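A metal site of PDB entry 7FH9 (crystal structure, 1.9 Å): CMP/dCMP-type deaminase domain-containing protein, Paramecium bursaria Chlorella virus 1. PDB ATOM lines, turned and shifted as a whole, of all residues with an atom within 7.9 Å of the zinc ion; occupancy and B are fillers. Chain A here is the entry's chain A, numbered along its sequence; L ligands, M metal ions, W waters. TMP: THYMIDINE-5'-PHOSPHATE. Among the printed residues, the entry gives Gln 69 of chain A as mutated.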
ATOM      1  N   VAL A  66      24.308 -10.125  10.280  1.00  0.00           N
ATOM      2  CA  VAL A  66      23.757 -11.299   9.602  1.00  0.00           C
ATOM      3  C   VAL A  66      24.344 -12.535  10.268  1.00  0.00           C
ATOM      4  O   VAL A  66      25.568 -12.604  10.474  1.00  0.00           O
ATOM      5  CB  VAL A  66      24.084 -11.295   8.099  1.00  0.00           C
ATOM      6  CG1 VAL A  66      23.517 -12.577   7.407  1.00  0.00           C
ATOM      7  CG2 VAL A  66      23.564 -10.012   7.412  1.00  0.00           C
ATOM      8  N   HIS A  67      23.495 -13.513  10.592  1.00  0.00           N
ATOM      9  CA  HIS A  67      23.971 -14.763  11.164  1.00  0.00           C
ATOM     10  C   HIS A  67      24.818 -15.547  10.168  1.00  0.00           C
ATOM     11  O   HIS A  67      24.620 -15.452   8.955  1.00  0.00           O
ATOM     12  CB  HIS A  67      22.780 -15.625  11.632  1.00  0.00           C
ATOM     13  CG  HIS A  67      22.143 -15.141  12.896  1.00  0.00           C
ATOM     14  ND1 HIS A  67      21.158 -15.858  13.551  1.00  0.00           N
ATOM     15  CD2 HIS A  67      22.345 -14.016  13.627  1.00  0.00           C
ATOM     16  CE1 HIS A  67      20.779 -15.190  14.632  1.00  0.00           C
ATOM     17  NE2 HIS A  67      21.491 -14.070  14.699  1.00  0.00           N
ATOM     18  N   ALA A  68      25.739 -16.353  10.697  1.00  0.00           N
ATOM     19  CA  ALA A  68      26.651 -17.096   9.825  1.00  0.00           C
ATOM     20  C   ALA A  68      25.897 -18.039   8.886  1.00  0.00           C
ATOM     21  O   ALA A  68      26.248 -18.160   7.704  1.00  0.00           O
ATOM     22  CB  ALA A  68      27.647 -17.892  10.677  1.00  0.00           C
ATOM     23  N   GLN A  69      24.882 -18.750   9.393  1.00  0.00           N
ATOM     24  CA  GLN A  69      24.240 -19.745   8.547  1.00  0.00           C
ATOM     25  C   GLN A  69      23.373 -19.077   7.478  1.00  0.00           C
ATOM     26  O   GLN A  69      23.418 -19.474   6.307  1.00  0.00           O
ATOM     27  CB  GLN A  69      23.462 -20.743   9.412  1.00  0.00           C
ATOM     28  CG  GLN A  69      24.464 -21.578  10.247  1.00  0.00           C
ATOM     29  CD  GLN A  69      23.853 -22.552  11.241  1.00  0.00           C
ATOM     30  OE1 GLN A  69      23.353 -23.613  10.865  1.00  0.00           O
ATOM     31  NE2 GLN A  69      23.917 -22.203  12.520  1.00  0.00           N
ATOM     32  N   ALA A  70      22.613 -18.036   7.851  1.00  0.00           N
ATOM     33  CA  ALA A  70      21.948 -17.208   6.852  1.00  0.00           C
ATOM     34  C   ALA A  70      22.923 -16.686   5.808  1.00  0.00           C
ATOM     35  O   ALA A  70      22.626 -16.706   4.600  1.00  0.00           O
ATOM     36  CB  ALA A  70      21.241 -16.031   7.527  1.00  0.00           C
ATOM     37  N   ASN A  71      24.103 -16.192   6.248  1.00  0.00           N
ATOM     38  CA  ASN A  71      25.083 -15.667   5.309  1.00  0.00           C
ATOM     39  C   ASN A  71      25.577 -16.737   4.343  1.00  0.00           C
ATOM     40  O   ASN A  71      25.808 -16.445   3.169  1.00  0.00           O
ATOM     41  CB  ASN A  71      26.284 -15.060   6.047  1.00  0.00           C
ATOM     42  CG  ASN A  71      26.388 -13.560   5.858  1.00  0.00           C
ATOM     43  OD1 ASN A  71      25.915 -13.019   4.851  1.00  0.00           O
ATOM     44  ND2 ASN A  71      27.033 -12.885   6.798  1.00  0.00           N
ATOM     45  N   LEU A  92      27.740 -23.157  15.682  1.00  0.00           N
ATOM     46  CA  LEU A  92      26.659 -22.861  16.617  1.00  0.00           C
ATOM     47  C   LEU A  92      25.366 -23.419  16.059  1.00  0.00           C
ATOM     48  O   LEU A  92      25.081 -23.215  14.880  1.00  0.00           O
ATOM     49  CB  LEU A  92      26.558 -21.341  16.840  1.00  0.00           C
ATOM     50  CG  LEU A  92      25.490 -20.798  17.767  1.00  0.00           C
ATOM     51  CD1 LEU A  92      25.737 -21.289  19.188  1.00  0.00           C
ATOM     52  CD2 LEU A  92      25.515 -19.258  17.703  1.00  0.00           C
ATOM     53  N   PHE A  93      24.588 -24.116  16.889  1.00  0.00           N
ATOM     54  CA  PHE A  93      23.317 -24.662  16.413  1.00  0.00           C
ATOM     55  C   PHE A  93      22.414 -23.517  15.945  1.00  0.00           C
ATOM     56  O   PHE A  93      22.332 -22.482  16.625  1.00  0.00           O
ATOM     57  CB  PHE A  93      22.625 -25.464  17.522  1.00  0.00           C
ATOM     58  CG  PHE A  93      21.380 -26.189  17.077  1.00  0.00           C
ATOM     59  CD1 PHE A  93      20.151 -25.536  17.030  1.00  0.00           C
ATOM     60  CD2 PHE A  93      21.437 -27.528  16.715  1.00  0.00           C
ATOM     61  CE1 PHE A  93      19.014 -26.205  16.620  1.00  0.00           C
ATOM     62  CE2 PHE A  93      20.284 -28.202  16.304  1.00  0.00           C
ATOM     63  CZ  PHE A  93      19.074 -27.535  16.256  1.00  0.00           C
ATOM     64  N   PRO A  94      21.720 -23.681  14.821  1.00  0.00           N
ATOM     65  CA  PRO A  94      21.004 -22.552  14.229  1.00  0.00           C
ATOM     66  C   PRO A  94      19.830 -22.059  15.058  1.00  0.00           C
ATOM     67  O   PRO A  94      19.128 -22.842  15.716  1.00  0.00           O
ATOM     68  CB  PRO A  94      20.515 -23.106  12.885  1.00  0.00           C
ATOM     69  CG  PRO A  94      20.465 -24.609  13.098  1.00  0.00           C
ATOM     70  CD  PRO A  94      21.648 -24.895  13.981  1.00  0.00           C
ATOM     71  N   CYS A  95      19.604 -20.753  14.993  1.00  0.00           N
ATOM     72  CA  CYS A  95      18.395 -20.172  15.556  1.00  0.00           C
ATOM     73  C   CYS A  95      17.179 -20.585  14.732  1.00  0.00           C
ATOM     74  O   CYS A  95      17.293 -21.174  13.647  1.00  0.00           O
ATOM     75  CB  CYS A  95      18.494 -18.640  15.611  1.00  0.00           C
ATOM     76  SG  CYS A  95      18.310 -17.809  13.979  1.00  0.00           S
ATOM     77  N   LYS A  96      15.993 -20.236  15.244  1.00  0.00           N
ATOM     78  CA  LYS A  96      14.741 -20.603  14.588  1.00  0.00           C
ATOM     79  C   LYS A  96      14.666 -20.082  13.160  1.00  0.00           C
ATOM     80  O   LYS A  96      14.222 -20.794  12.255  1.00  0.00           O
ATOM     81  CB  LYS A  96      13.566 -20.089  15.417  1.00  0.00           C
ATOM     82  CG  LYS A  96      12.207 -20.515  14.927  1.00  0.00           C
ATOM     83  CD  LYS A  96      11.117 -20.140  15.941  1.00  0.00           C
ATOM     84  CE  LYS A  96      10.948 -18.638  16.077  1.00  0.00           C
ATOM     85  NZ  LYS A  96      10.009 -18.301  17.170  1.00  0.00           N
ATOM     86  N   GLU A  97      15.091 -18.829  12.926  1.00  0.00           N
ATOM     87  CA  GLU A  97      14.967 -18.279  11.579  1.00  0.00           C
ATOM     88  C   GLU A  97      15.965 -18.903  10.615  1.00  0.00           C
ATOM     89  O   GLU A  97      15.618 -19.197   9.465  1.00  0.00           O
ATOM     90  CB  GLU A  97      15.116 -16.750  11.613  1.00  0.00           C
ATOM     91  CG  GLU A  97      14.194 -16.085  12.634  1.00  0.00           C
ATOM     92  CD  GLU A  97      12.697 -16.280  12.321  1.00  0.00           C
ATOM     93  OE1 GLU A  97      12.384 -16.673  11.184  1.00  0.00           O
ATOM     94  OE2 GLU A  97      11.863 -16.036  13.212  1.00  0.00           O
ATOM     95  N   CYS A  98      17.203 -19.105  11.053  1.00  0.00           N
ATOM     96  CA  CYS A  98      18.176 -19.772  10.189  1.00  0.00           C
ATOM     97  C   CYS A  98      17.774 -21.203   9.892  1.00  0.00           C
ATOM     98  O   CYS A  98      18.047 -21.713   8.798  1.00  0.00           O
ATOM     99  CB  CYS A  98      19.573 -19.731  10.821  1.00  0.00           C
ATOM    100  SG  CYS A  98      20.398 -18.083  10.754  1.00  0.00           S
ATOM    101  N   SER A  99      17.123 -21.886  10.842  1.00  0.00           N
ATOM    102  CA  SER A  99      16.637 -23.244  10.576  1.00  0.00           C
ATOM    103  C   SER A  99      15.635 -23.254   9.417  1.00  0.00           C
ATOM    104  O   SER A  99      15.668 -24.148   8.566  1.00  0.00           O
ATOM    105  CB  SER A  99      16.006 -23.833  11.836  1.00  0.00           C
ATOM    106  OG  SER A  99      16.980 -23.970  12.858  1.00  0.00           O
ATOM    107  N   LEU A 101      15.601 -21.144   6.894  1.00  0.00           N
ATOM    108  CA  LEU A 101      16.349 -20.902   5.664  1.00  0.00           C
ATOM    109  C   LEU A 101      17.153 -22.135   5.261  1.00  0.00           C
ATOM    110  O   LEU A 101      17.304 -22.412   4.068  1.00  0.00           O
ATOM    111  CB  LEU A 101      17.289 -19.715   5.820  1.00  0.00           C
ATOM    112  CG  LEU A 101      16.597 -18.386   6.172  1.00  0.00           C
ATOM    113  CD1 LEU A 101      17.642 -17.318   6.366  1.00  0.00           C
ATOM    114  CD2 LEU A 101      15.573 -17.986   5.112  1.00  0.00           C
ATOM    115  N   ILE A 102      17.680 -22.858   6.243  1.00  0.00           N
ATOM    116  CA  ILE A 102      18.381 -24.113   5.981  1.00  0.00           C
ATOM    117  C   ILE A 102      17.466 -25.084   5.244  1.00  0.00           C
ATOM    118  O   ILE A 102      17.853 -25.713   4.243  1.00  0.00           O
ATOM    119  CB  ILE A 102      18.921 -24.716   7.280  1.00  0.00           C
ATOM    120  CG1 ILE A 102      20.130 -23.921   7.772  1.00  0.00           C
ATOM    121  CG2 ILE A 102      19.251 -26.226   7.095  1.00  0.00           C
ATOM    122  CD1 ILE A 102      20.514 -24.221   9.199  1.00  0.00           C
ATOM    123  N   TRP A 121      16.773 -20.229  25.474  1.00  0.00           N
ATOM    124  CA  TRP A 121      16.783 -20.730  24.098  1.00  0.00           C
ATOM    125  C   TRP A 121      16.003 -22.030  23.920  1.00  0.00           C
ATOM    126  O   TRP A 121      15.959 -22.564  22.808  1.00  0.00           O
ATOM    127  CB  TRP A 121      18.214 -20.936  23.615  1.00  0.00           C
ATOM    128  CG  TRP A 121      18.915 -19.670  23.245  1.00  0.00           C
ATOM    129  CD1 TRP A 121      19.718 -18.913  24.056  1.00  0.00           C
ATOM    130  CD2 TRP A 121      18.877 -18.999  21.985  1.00  0.00           C
ATOM    131  NE1 TRP A 121      20.179 -17.813  23.365  1.00  0.00           N
ATOM    132  CE2 TRP A 121      19.683 -17.841  22.085  1.00  0.00           C
ATOM    133  CE3 TRP A 121      18.243 -19.267  20.761  1.00  0.00           C
ATOM    134  CZ2 TRP A 121      19.868 -16.961  21.026  1.00  0.00           C
ATOM    135  CZ3 TRP A 121      18.426 -18.383  19.715  1.00  0.00           C
ATOM    136  CH2 TRP A 121      19.232 -17.248  19.852  1.00  0.00           C
HETATM  137  P   TMP L   1      26.716 -11.592  21.348  1.00  0.00           P
HETATM  138  O1P TMP L   1      27.409 -12.858  21.800  1.00  0.00           O
HETATM  139  O2P TMP L   1      27.443 -10.334  21.802  1.00  0.00           O
HETATM  140  O3P TMP L   1      25.238 -11.564  21.671  1.00  0.00           O
HETATM  141  O5' TMP L   1      26.810 -11.591  19.737  1.00  0.00           O
HETATM  142  C5' TMP L   1      26.417 -12.784  19.013  1.00  0.00           C
HETATM  143  C4' TMP L   1      26.949 -12.714  17.602  1.00  0.00           C
HETATM  144  O4' TMP L   1      26.777 -13.996  16.948  1.00  0.00           O
HETATM  145  C3' TMP L   1      26.262 -11.687  16.702  1.00  0.00           C
HETATM  146  O3' TMP L   1      27.185 -11.150  15.765  1.00  0.00           O
HETATM  147  C2' TMP L   1      25.198 -12.524  16.005  1.00  0.00           C
HETATM  148  C1' TMP L   1      25.885 -13.879  15.848  1.00  0.00           C
HETATM  149  N1  TMP L   1      24.966 -15.033  15.894  1.00  0.00           N
HETATM  150  C2  TMP L   1      24.963 -15.902  14.828  1.00  0.00           C
HETATM  151  O2  TMP L   1      25.694 -15.754  13.849  1.00  0.00           O
HETATM  152  N3  TMP L   1      24.088 -16.948  14.929  1.00  0.00           N
HETATM  153  C4  TMP L   1      23.233 -17.204  15.990  1.00  0.00           C
HETATM  154  O4  TMP L   1      22.489 -18.195  15.944  1.00  0.00           O
HETATM  155  C5  TMP L   1      23.279 -16.258  17.077  1.00  0.00           C
HETATM  156  C5M TMP L   1      22.385 -16.466  18.259  1.00  0.00           C
HETATM  157  C6  TMP L   1      24.134 -15.225  16.976  1.00  0.00           C
HETATM  158 ZN    ZN M   1      20.318 -17.586  12.945  1.00  0.00          ZN
HETATM  159  O   HOH W   1      21.650 -18.995  13.764  1.00  0.00           O
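SG of Cys 98 sits close to N of Ala 70 (3.7 Å). The backbone carbonyl oxygen of Cys 95 sits at hydrogen-bond distance from the side-chain hydroxyl of Ser 99 (2.9 Å). The side-chain sulfur of Cys 95 lies close to the backbone NH of Glu 97, 3.5 Å away.
O2 of the ligand sits at hydrogen-bond distance from N of Ala 68 (3.2 Å). A ring nitrogen (ND1) of His 67 sits close to a nitrogen (N3) of the ligand (3.4 Å).
Of the 17 residues printed, 3 come within 4 Å of the zinc ion. The nearest printed residue that does not touch the zinc ion is Pro 94 (5.0 Å).
The zinc ion is bound by a ring nitrogen (ND1) of His 67, water W1, the side-chain sulfur of Cys 98 and the side-chain sulfur of Cys 95. The zinc ion has four donor atoms within binding distance.
Water W1 lies within hydrogen-bond range of an oxygen (O4) of the ligand (2.5 Å) and the backbone NH (N) of Cys 95 (3.0 Å).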
